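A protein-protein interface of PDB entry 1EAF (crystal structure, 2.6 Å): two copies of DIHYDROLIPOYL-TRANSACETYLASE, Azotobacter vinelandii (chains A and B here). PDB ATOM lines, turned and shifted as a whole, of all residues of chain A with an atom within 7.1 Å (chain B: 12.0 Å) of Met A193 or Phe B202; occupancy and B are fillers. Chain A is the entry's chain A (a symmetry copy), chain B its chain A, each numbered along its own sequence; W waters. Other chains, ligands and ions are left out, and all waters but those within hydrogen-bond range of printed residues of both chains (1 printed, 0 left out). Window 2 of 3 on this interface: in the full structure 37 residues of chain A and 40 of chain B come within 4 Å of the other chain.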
ATOM      1  N   THR A  50      -8.894   6.041 -24.523  1.00  0.00           N
ATOM      2  CA  THR A  50      -8.067   7.220 -24.220  1.00  0.00           C
ATOM      3  C   THR A  50      -6.962   7.457 -25.247  1.00  0.00           C
ATOM      4  O   THR A  50      -6.810   8.551 -25.785  1.00  0.00           O
ATOM      5  CB  THR A  50      -7.447   7.041 -22.806  1.00  0.00           C
ATOM      6  OG1 THR A  50      -8.501   6.669 -21.939  1.00  0.00           O
ATOM      7  CG2 THR A  50      -6.826   8.298 -22.247  1.00  0.00           C
ATOM      8  N   ALA A 191     -19.055   8.621 -25.690  1.00  0.00           N
ATOM      9  CA  ALA A 191     -17.923   8.327 -24.821  1.00  0.00           C
ATOM     10  C   ALA A 191     -17.912   9.332 -23.682  1.00  0.00           C
ATOM     11  O   ALA A 191     -18.290  10.498 -23.866  1.00  0.00           O
ATOM     12  CB  ALA A 191     -16.619   8.490 -25.519  1.00  0.00           C
ATOM     13  N   SER A 192     -17.526   8.921 -22.483  1.00  0.00           N
ATOM     14  CA  SER A 192     -17.378   9.859 -21.395  1.00  0.00           C
ATOM     15  C   SER A 192     -16.252   9.368 -20.517  1.00  0.00           C
ATOM     16  O   SER A 192     -15.849   8.206 -20.545  1.00  0.00           O
ATOM     17  CB  SER A 192     -18.682   9.916 -20.644  1.00  0.00           C
ATOM     18  OG  SER A 192     -18.937   8.703 -19.959  1.00  0.00           O
ATOM     19  N   MET A 193     -15.720  10.310 -19.779  1.00  0.00           N
ATOM     20  CA  MET A 193     -14.671  10.116 -18.786  1.00  0.00           C
ATOM     21  C   MET A 193     -15.169   9.331 -17.589  1.00  0.00           C
ATOM     22  O   MET A 193     -16.112   9.790 -16.957  1.00  0.00           O
ATOM     23  CB  MET A 193     -14.197  11.469 -18.359  1.00  0.00           C
ATOM     24  CG  MET A 193     -12.752  11.405 -18.137  1.00  0.00           C
ATOM     25  SD  MET A 193     -11.880  11.458 -19.720  1.00  0.00           S
ATOM     26  CE  MET A 193     -10.511  10.813 -18.852  1.00  0.00           C
ATOM     27  N   GLN A 194     -14.571   8.199 -17.243  1.00  0.00           N
ATOM     28  CA  GLN A 194     -15.025   7.335 -16.161  1.00  0.00           C
ATOM     29  C   GLN A 194     -13.853   6.970 -15.270  1.00  0.00           C
ATOM     30  O   GLN A 194     -12.727   6.952 -15.758  1.00  0.00           O
ATOM     31  CB  GLN A 194     -15.612   6.031 -16.700  1.00  0.00           C
ATOM     32  CG  GLN A 194     -16.900   6.145 -17.528  1.00  0.00           C
ATOM     33  CD  GLN A 194     -17.999   6.861 -16.750  1.00  0.00           C
ATOM     34  OE1 GLN A 194     -18.190   6.623 -15.540  1.00  0.00           O
ATOM     35  NE2 GLN A 194     -18.731   7.764 -17.403  1.00  0.00           N
ATOM     36  N   PRO A 195     -14.011   6.699 -13.979  1.00  0.00           N
ATOM     37  CA  PRO A 195     -12.943   6.239 -13.124  1.00  0.00           C
ATOM     38  C   PRO A 195     -12.792   4.755 -13.272  1.00  0.00           C
ATOM     39  O   PRO A 195     -13.750   4.007 -13.089  1.00  0.00           O
ATOM     40  CB  PRO A 195     -13.336   6.650 -11.754  1.00  0.00           C
ATOM     41  CG  PRO A 195     -14.825   6.573 -11.811  1.00  0.00           C
ATOM     42  CD  PRO A 195     -15.181   7.043 -13.197  1.00  0.00           C
ATOM     43  N   VAL A 196     -11.591   4.337 -13.621  1.00  0.00           N
ATOM     44  CA  VAL A 196     -11.290   2.960 -13.886  1.00  0.00           C
ATOM     45  C   VAL A 196     -10.177   2.596 -12.906  1.00  0.00           C
ATOM     46  O   VAL A 196      -9.218   3.351 -12.688  1.00  0.00           O
ATOM     47  CB  VAL A 196     -10.860   2.861 -15.344  1.00  0.00           C
ATOM     48  CG1 VAL A 196     -10.629   1.432 -15.661  1.00  0.00           C
ATOM     49  CG2 VAL A 196     -11.926   3.343 -16.280  1.00  0.00           C
ATOM     50  N   PHE A 202      -8.402   4.870  -8.863  1.00  0.00           N
ATOM     51  CA  PHE A 202      -9.219   5.081 -10.032  1.00  0.00           C
ATOM     52  C   PHE A 202      -8.512   6.150 -10.827  1.00  0.00           C
ATOM     53  O   PHE A 202      -8.147   7.158 -10.245  1.00  0.00           O
ATOM     54  CB  PHE A 202     -10.621   5.575  -9.652  1.00  0.00           C
ATOM     55  CG  PHE A 202     -11.448   4.507  -8.954  1.00  0.00           C
ATOM     56  CD1 PHE A 202     -12.009   3.497  -9.718  1.00  0.00           C
ATOM     57  CD2 PHE A 202     -11.603   4.514  -7.577  1.00  0.00           C
ATOM     58  CE1 PHE A 202     -12.718   2.489  -9.100  1.00  0.00           C
ATOM     59  CE2 PHE A 202     -12.310   3.512  -6.961  1.00  0.00           C
ATOM     60  CZ  PHE A 202     -12.864   2.501  -7.725  1.00  0.00           C
ATOM     61  N   GLN A 203      -8.226   5.895 -12.099  1.00  0.00           N
ATOM     62  CA  GLN A 203      -7.658   6.850 -13.045  1.00  0.00           C
ATOM     63  C   GLN A 203      -8.801   7.353 -13.925  1.00  0.00           C
ATOM     64  O   GLN A 203      -9.710   6.553 -14.192  1.00  0.00           O
ATOM     65  CB  GLN A 203      -6.630   6.178 -13.938  1.00  0.00           C
ATOM     66  CG  GLN A 203      -5.472   5.617 -13.149  1.00  0.00           C
ATOM     67  CD  GLN A 203      -4.786   6.647 -12.242  1.00  0.00           C
ATOM     68  OE1 GLN A 203      -4.677   7.831 -12.565  1.00  0.00           O
ATOM     69  NE2 GLN A 203      -4.273   6.322 -11.055  1.00  0.00           N
ATOM     70  N   PRO A 204      -8.892   8.589 -14.443  1.00  0.00           N
ATOM     71  CA  PRO A 204      -9.873   8.932 -15.471  1.00  0.00           C
ATOM     72  C   PRO A 204      -9.522   8.357 -16.830  1.00  0.00           C
ATOM     73  O   PRO A 204      -8.444   8.688 -17.332  1.00  0.00           O
ATOM     74  CB  PRO A 204      -9.923  10.434 -15.446  1.00  0.00           C
ATOM     75  CG  PRO A 204      -8.588  10.865 -14.881  1.00  0.00           C
ATOM     76  CD  PRO A 204      -8.177   9.749 -13.938  1.00  0.00           C
ATOM     77  N   ARG A 205     -10.371   7.508 -17.450  1.00  0.00           N
ATOM     78  CA  ARG A 205     -10.159   6.941 -18.778  1.00  0.00           C
ATOM     79  C   ARG A 205     -11.353   7.315 -19.633  1.00  0.00           C
ATOM     80  O   ARG A 205     -12.474   7.398 -19.081  1.00  0.00           O
ATOM     81  CB  ARG A 205     -10.060   5.433 -18.725  1.00  0.00           C
ATOM     82  CG  ARG A 205      -8.988   4.989 -17.744  1.00  0.00           C
ATOM     83  CD  ARG A 205      -7.608   5.530 -18.155  1.00  0.00           C
ATOM     84  NE  ARG A 205      -7.130   4.780 -19.294  1.00  0.00           N
ATOM     85  CZ  ARG A 205      -6.062   5.088 -20.052  1.00  0.00           C
ATOM     86  NH1 ARG A 205      -5.271   6.131 -19.735  1.00  0.00           N
ATOM     87  NH2 ARG A 205      -5.750   4.296 -21.104  1.00  0.00           N
ATOM     88  N   LEU A 206     -11.168   7.615 -20.930  1.00  0.00           N
ATOM     89  CA  LEU A 206     -12.311   7.930 -21.787  1.00  0.00           C
ATOM     90  C   LEU A 206     -12.923   6.611 -22.248  1.00  0.00           C
ATOM     91  O   LEU A 206     -12.252   5.837 -22.943  1.00  0.00           O
ATOM     92  CB  LEU A 206     -11.870   8.727 -22.992  1.00  0.00           C
ATOM     93  CG  LEU A 206     -12.932   9.254 -23.957  1.00  0.00           C
ATOM     94  CD1 LEU A 206     -13.783  10.299 -23.264  1.00  0.00           C
ATOM     95  CD2 LEU A 206     -12.263   9.903 -25.158  1.00  0.00           C
ATOM     96  N   MET A 207     -14.143   6.295 -21.826  1.00  0.00           N
ATOM     97  CA  MET A 207     -14.753   4.994 -22.113  1.00  0.00           C
ATOM     98  C   MET A 207     -15.855   5.109 -23.148  1.00  0.00           C
ATOM     99  O   MET A 207     -16.688   6.029 -23.098  1.00  0.00           O
ATOM    100  CB  MET A 207     -15.349   4.384 -20.851  1.00  0.00           C
ATOM    101  CG  MET A 207     -14.370   4.198 -19.718  1.00  0.00           C
ATOM    102  SD  MET A 207     -12.972   3.096 -20.079  1.00  0.00           S
ATOM    103  CE  MET A 207     -13.739   1.516 -20.028  1.00  0.00           C
ATOM    104  N   GLU B  45     -29.952   6.522 -20.527  1.00  0.00           N
ATOM    105  CA  GLU B  45     -29.356   7.838 -20.307  1.00  0.00           C
ATOM    106  C   GLU B  45     -29.291   8.069 -18.800  1.00  0.00           C
ATOM    107  O   GLU B  45     -30.103   7.471 -18.097  1.00  0.00           O
ATOM    108  CB  GLU B  45     -30.236   8.929 -20.929  1.00  0.00           C
ATOM    109  CG  GLU B  45     -29.788  10.386 -20.760  1.00  0.00           C
ATOM    110  CD  GLU B  45     -28.454  10.607 -21.466  1.00  0.00           C
ATOM    111  OE1 GLU B  45     -27.358  10.329 -20.944  1.00  0.00           O
ATOM    112  OE2 GLU B  45     -28.508  10.990 -22.615  1.00  0.00           O
ATOM    113  N   SER B  46     -28.422   8.916 -18.256  1.00  0.00           N
ATOM    114  CA  SER B  46     -28.461   9.235 -16.829  1.00  0.00           C
ATOM    115  C   SER B  46     -28.643  10.719 -16.731  1.00  0.00           C
ATOM    116  O   SER B  46     -27.912  11.406 -17.454  1.00  0.00           O
ATOM    117  CB  SER B  46     -27.196   8.932 -16.126  1.00  0.00           C
ATOM    118  OG  SER B  46     -27.272   7.540 -15.970  1.00  0.00           O
ATOM    119  N   ASP B  48     -28.538  14.263 -14.401  1.00  0.00           N
ATOM    120  CA  ASP B  48     -27.977  14.746 -13.161  1.00  0.00           C
ATOM    121  C   ASP B  48     -29.095  15.452 -12.442  1.00  0.00           C
ATOM    122  O   ASP B  48     -29.494  16.541 -12.887  1.00  0.00           O
ATOM    123  CB  ASP B  48     -26.868  15.714 -13.446  1.00  0.00           C
ATOM    124  CG  ASP B  48     -26.167  16.308 -12.225  1.00  0.00           C
ATOM    125  OD1 ASP B  48     -26.695  16.405 -11.115  1.00  0.00           O
ATOM    126  OD2 ASP B  48     -25.025  16.689 -12.420  1.00  0.00           O
ATOM    127  N   THR B  50     -28.976  16.526  -9.111  1.00  0.00           N
ATOM    128  CA  THR B  50     -28.528  17.076  -7.822  1.00  0.00           C
ATOM    129  C   THR B  50     -29.327  18.301  -7.381  1.00  0.00           C
ATOM    130  O   THR B  50     -29.832  18.369  -6.264  1.00  0.00           O
ATOM    131  CB  THR B  50     -27.021  17.438  -7.934  1.00  0.00           C
ATOM    132  OG1 THR B  50     -26.368  16.316  -8.495  1.00  0.00           O
ATOM    133  CG2 THR B  50     -26.361  17.727  -6.607  1.00  0.00           C
ATOM    134  N   MET B 193     -25.643   8.320  -6.134  1.00  0.00           N
ATOM    135  CA  MET B 193     -24.467   9.179  -6.180  1.00  0.00           C
ATOM    136  C   MET B 193     -23.383   8.601  -7.066  1.00  0.00           C
ATOM    137  O   MET B 193     -22.945   7.493  -6.783  1.00  0.00           O
ATOM    138  CB  MET B 193     -23.966   9.335  -4.779  1.00  0.00           C
ATOM    139  CG  MET B 193     -23.472  10.702  -4.613  1.00  0.00           C
ATOM    140  SD  MET B 193     -24.861  11.837  -4.378  1.00  0.00           S
ATOM    141  CE  MET B 193     -23.744  13.105  -4.814  1.00  0.00           C
ATOM    142  N   GLN B 194     -22.923   9.301  -8.094  1.00  0.00           N
ATOM    143  CA  GLN B 194     -21.942   8.799  -9.048  1.00  0.00           C
ATOM    144  C   GLN B 194     -20.841   9.826  -9.240  1.00  0.00           C
ATOM    145  O   GLN B 194     -21.106  11.011  -9.063  1.00  0.00           O
ATOM    146  CB  GLN B 194     -22.575   8.547 -10.416  1.00  0.00           C
ATOM    147  CG  GLN B 194     -23.634   7.438 -10.491  1.00  0.00           C
ATOM    148  CD  GLN B 194     -23.083   6.110  -9.984  1.00  0.00           C
ATOM    149  OE1 GLN B 194     -21.930   5.735 -10.281  1.00  0.00           O
ATOM    150  NE2 GLN B 194     -23.868   5.375  -9.196  1.00  0.00           N
ATOM    151  N   PRO B 195     -19.603   9.474  -9.567  1.00  0.00           N
ATOM    152  CA  PRO B 195     -18.557  10.423  -9.868  1.00  0.00           C
ATOM    153  C   PRO B 195     -18.665  10.841 -11.304  1.00  0.00           C
ATOM    154  O   PRO B 195     -18.664  10.002 -12.202  1.00  0.00           O
ATOM    155  CB  PRO B 195     -17.290   9.716  -9.562  1.00  0.00           C
ATOM    156  CG  PRO B 195     -17.629   8.298  -9.878  1.00  0.00           C
ATOM    157  CD  PRO B 195     -19.060   8.137  -9.438  1.00  0.00           C
ATOM    158  N   VAL B 196     -18.777  12.138 -11.511  1.00  0.00           N
ATOM    159  CA  VAL B 196     -18.972  12.706 -12.813  1.00  0.00           C
ATOM    160  C   VAL B 196     -17.795  13.659 -13.016  1.00  0.00           C
ATOM    161  O   VAL B 196     -17.404  14.423 -12.122  1.00  0.00           O
ATOM    162  CB  VAL B 196     -20.320  13.414 -12.804  1.00  0.00           C
ATOM    163  CG1 VAL B 196     -20.579  13.933 -14.167  1.00  0.00           C
ATOM    164  CG2 VAL B 196     -21.445  12.480 -12.478  1.00  0.00           C
ATOM    165  N   TRP B 197     -17.141  13.522 -14.168  1.00  0.00           N
ATOM    166  CA  TRP B 197     -15.977  14.325 -14.502  1.00  0.00           C
ATOM    167  C   TRP B 197     -16.361  15.766 -14.774  1.00  0.00           C
ATOM    168  O   TRP B 197     -17.201  15.990 -15.640  1.00  0.00           O
ATOM    169  CB  TRP B 197     -15.322  13.781 -15.734  1.00  0.00           C
ATOM    170  CG  TRP B 197     -13.982  14.395 -16.135  1.00  0.00           C
ATOM    171  CD1 TRP B 197     -13.842  15.108 -17.313  1.00  0.00           C
ATOM    172  CD2 TRP B 197     -12.787  14.195 -15.480  1.00  0.00           C
ATOM    173  NE1 TRP B 197     -12.547  15.311 -17.393  1.00  0.00           N
ATOM    174  CE2 TRP B 197     -11.896  14.786 -16.340  1.00  0.00           C
ATOM    175  CE3 TRP B 197     -12.358  13.589 -14.319  1.00  0.00           C
ATOM    176  CZ2 TRP B 197     -10.559  14.779 -16.051  1.00  0.00           C
ATOM    177  CZ3 TRP B 197     -11.019  13.575 -14.018  1.00  0.00           C
ATOM    178  CH2 TRP B 197     -10.129  14.174 -14.888  1.00  0.00           C
ATOM    179  N   ASP B 198     -15.741  16.749 -14.128  1.00  0.00           N
ATOM    180  CA  ASP B 198     -16.123  18.123 -14.432  1.00  0.00           C
ATOM    181  C   ASP B 198     -15.172  18.750 -15.423  1.00  0.00           C
ATOM    182  O   ASP B 198     -15.251  19.943 -15.709  1.00  0.00           O
ATOM    183  CB  ASP B 198     -16.154  19.015 -13.180  1.00  0.00           C
ATOM    184  CG  ASP B 198     -14.865  19.094 -12.379  1.00  0.00           C
ATOM    185  OD1 ASP B 198     -13.780  18.950 -12.927  1.00  0.00           O
ATOM    186  OD2 ASP B 198     -14.940  19.315 -11.177  1.00  0.00           O
ATOM    187  N   GLY B 199     -14.170  17.996 -15.856  1.00  0.00           N
ATOM    188  CA  GLY B 199     -13.193  18.519 -16.776  1.00  0.00           C
ATOM    189  C   GLY B 199     -11.850  18.404 -16.131  1.00  0.00           C
ATOM    190  O   GLY B 199     -10.855  18.390 -16.837  1.00  0.00           O
ATOM    191  N   LYS B 200     -11.803  18.181 -14.825  1.00  0.00           N
ATOM    192  CA  LYS B 200     -10.560  18.232 -14.086  1.00  0.00           C
ATOM    193  C   LYS B 200     -10.589  17.208 -12.968  1.00  0.00           C
ATOM    194  O   LYS B 200      -9.548  16.725 -12.522  1.00  0.00           O
ATOM    195  CB  LYS B 200     -10.419  19.643 -13.514  1.00  0.00           C
ATOM    196  CG  LYS B 200      -9.185  20.008 -12.662  1.00  0.00           C
ATOM    197  CD  LYS B 200      -7.916  20.092 -13.569  1.00  0.00           C
ATOM    198  CE  LYS B 200      -6.657  20.902 -13.063  1.00  0.00           C
ATOM    199  NZ  LYS B 200      -5.699  21.120 -14.160  1.00  0.00           N
ATOM    200  N   ALA B 201     -11.760  16.882 -12.401  1.00  0.00           N
ATOM    201  CA  ALA B 201     -11.887  15.908 -11.310  1.00  0.00           C
ATOM    202  C   ALA B 201     -13.299  15.323 -11.304  1.00  0.00           C
ATOM    203  O   ALA B 201     -14.194  15.847 -11.975  1.00  0.00           O
ATOM    204  CB  ALA B 201     -11.658  16.566  -9.955  1.00  0.00           C
ATOM    205  N   PHE B 202     -13.502  14.240 -10.588  1.00  0.00           N
ATOM    206  CA  PHE B 202     -14.807  13.635 -10.484  1.00  0.00           C
ATOM    207  C   PHE B 202     -15.458  14.293  -9.294  1.00  0.00           C
ATOM    208  O   PHE B 202     -14.824  14.371  -8.255  1.00  0.00           O
ATOM    209  CB  PHE B 202     -14.703  12.125 -10.234  1.00  0.00           C
ATOM    210  CG  PHE B 202     -14.169  11.368 -11.441  1.00  0.00           C
ATOM    211  CD1 PHE B 202     -15.020  11.136 -12.508  1.00  0.00           C
ATOM    212  CD2 PHE B 202     -12.847  10.957 -11.495  1.00  0.00           C
ATOM    213  CE1 PHE B 202     -14.542  10.499 -13.633  1.00  0.00           C
ATOM    214  CE2 PHE B 202     -12.371  10.321 -12.613  1.00  0.00           C
ATOM    215  CZ  PHE B 202     -13.220  10.095 -13.681  1.00  0.00           C
ATOM    216  N   GLN B 203     -16.651  14.853  -9.466  1.00  0.00           N
ATOM    217  CA  GLN B 203     -17.477  15.424  -8.407  1.00  0.00           C
ATOM    218  C   GLN B 203     -18.562  14.400  -8.075  1.00  0.00           C
ATOM    219  O   GLN B 203     -18.992  13.703  -9.004  1.00  0.00           O
ATOM    220  CB  GLN B 203     -18.155  16.698  -8.880  1.00  0.00           C
ATOM    221  CG  GLN B 203     -17.156  17.763  -9.265  1.00  0.00           C
ATOM    222  CD  GLN B 203     -16.141  18.086  -8.161  1.00  0.00           C
ATOM    223  OE1 GLN B 203     -16.444  18.058  -6.967  1.00  0.00           O
ATOM    224  NE2 GLN B 203     -14.876  18.412  -8.429  1.00  0.00           N
ATOM    225  N   PRO B 204     -19.095  14.206  -6.857  1.00  0.00           N
ATOM    226  CA  PRO B 204     -20.293  13.394  -6.652  1.00  0.00           C
ATOM    227  C   PRO B 204     -21.557  14.085  -7.127  1.00  0.00           C
ATOM    228  O   PRO B 204     -21.846  15.169  -6.612  1.00  0.00           O
ATOM    229  CB  PRO B 204     -20.286  13.094  -5.180  1.00  0.00           C
ATOM    230  CG  PRO B 204     -19.480  14.208  -4.551  1.00  0.00           C
ATOM    231  CD  PRO B 204     -18.470  14.613  -5.609  1.00  0.00           C
ATOM    232  N   ARG B 205     -22.322  13.520  -8.087  1.00  0.00           N
ATOM    233  CA  ARG B 205     -23.582  14.069  -8.578  1.00  0.00           C
ATOM    234  C   ARG B 205     -24.650  13.013  -8.381  1.00  0.00           C
ATOM    235  O   ARG B 205     -24.323  11.810  -8.496  1.00  0.00           O
ATOM    236  CB  ARG B 205     -23.502  14.403 -10.050  1.00  0.00           C
ATOM    237  CG  ARG B 205     -22.333  15.329 -10.339  1.00  0.00           C
ATOM    238  CD  ARG B 205     -22.477  16.654  -9.570  1.00  0.00           C
ATOM    239  NE  ARG B 205     -23.500  17.455 -10.203  1.00  0.00           N
ATOM    240  CZ  ARG B 205     -24.043  18.581  -9.705  1.00  0.00           C
ATOM    241  NH1 ARG B 205     -23.586  19.115  -8.556  1.00  0.00           N
ATOM    242  NH2 ARG B 205     -25.011  19.212 -10.409  1.00  0.00           N
ATOM    243  N   LEU B 206     -25.891  13.388  -8.022  1.00  0.00           N
ATOM    244  CA  LEU B 206     -26.952  12.391  -7.875  1.00  0.00           C
ATOM    245  C   LEU B 206     -27.513  12.102  -9.264  1.00  0.00           C
ATOM    246  O   LEU B 206     -28.063  13.011  -9.900  1.00  0.00           O
ATOM    247  CB  LEU B 206     -28.056  12.914  -6.985  1.00  0.00           C
ATOM    248  CG  LEU B 206     -29.208  11.981  -6.614  1.00  0.00           C
ATOM    249  CD1 LEU B 206     -28.695  10.854  -5.740  1.00  0.00           C
ATOM    250  CD2 LEU B 206     -30.263  12.749  -5.834  1.00  0.00           C
ATOM    251  N   MET B 207     -27.329  10.894  -9.784  1.00  0.00           N
ATOM    252  CA  MET B 207     -27.719  10.572 -11.160  1.00  0.00           C
ATOM    253  C   MET B 207     -28.946   9.682 -11.198  1.00  0.00           C
ATOM    254  O   MET B 207     -29.060   8.714 -10.428  1.00  0.00           O
ATOM    255  CB  MET B 207     -26.591   9.857 -11.890  1.00  0.00           C
ATOM    256  CG  MET B 207     -25.290  10.621 -11.944  1.00  0.00           C
ATOM    257  SD  MET B 207     -25.372  12.224 -12.795  1.00  0.00           S
ATOM    258  CE  MET B 207     -25.459  11.733 -14.479  1.00  0.00           C
HETATM  259  O   HOH W   1     -18.089  11.677 -16.179  1.00  0.00           O
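The side-chain hydroxyl (OG) of Ser A192 sits at hydrogen-bond distance from the side-chain amide nitrogen (NE2) of Gln A194 (2.7 Å).
N of Gln A194 lies within hydrogen-bond range of O of Arg A205.
Printed residues of chain A that touch a printed residue of chain B: Met A193, Gln A194, Pro A195 and Pro A204.
Hydrophobic or aromatic side chains of chain A within 4 Å of the printed part of chain B: Met A193, Pro A195 and Pro A204.
Among the printed residues, 7 pairs touch across the chains.
Among the printed residues, no Asp or Glu carboxylate lies within 4 Å of a Lys or Arg side-chain nitrogen of the other chain.
Met A193 touches Phe B202, but with the chains exchanged Phe A202 does not touch Met B193 (11.3 Å).
Pro B195 touches its own counterpart, Pro A195.
Pro A195 touches Phe B202, but with the chains exchanged Phe A202 does not touch Pro B195 (7.3 Å).
Pro A204 touches Phe B202, but with the chains exchanged Phe A202 does not touch Pro B204 (12.3 Å).
Of the 7 pairs that touch across the chains among the printed residues, 1 has its exchanged pair printed and touching as well.
Water W1 lies within hydrogen-bond range of the backbone carbonyl oxygen of Met A193 (2.8 Å) and the backbone NH of Trp B197 (2.9 Å).
CB of Met A193 touches CB of Trp B197 (3.7 Å).
Phe B202 touches Met A193.
CZ of Phe B202 touches C of Gln A194 (3.6 Å).
Pro A195 touches Pro B195.
Pro A195 touches Phe B202 (N to CZ, 3.5 Å).
Trp B197 touches Pro A204.
CB of Pro A204 touches CE2 of Phe B202, 3.7 Å away.
Met A193 touches just these residues of chain B: Trp B197 (3.7 Å) and Phe B202 (3.7 Å).
Phe B202 touches four residues of chain A.
No residue of chain B comes within 4 Å of Ser A192.
Of chain B, only Pro B195 and Phe B202 come within 4 Å of Pro A195.
Of chain B, only Trp B197 and Phe B202 come within 4 Å of Pro A204.
Printed residues of chain A within 4 Å of Trp B197: Met A193 (3.7 Å) and Pro A204 (3.6 Å).
Of the printed residues of chain A, Pro B195 touches Pro A195 (3.8 Å).
Met B193 touches none of the printed residues of chain A.
Gln B203 touches none of the printed residues of chain A.
The nearest residue of chain B that does not touch Met A193 is Pro B195 (5.4 Å).
The nearest residue of chain A that does not touch Phe B202 is Gln A203 (4.8 Å).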
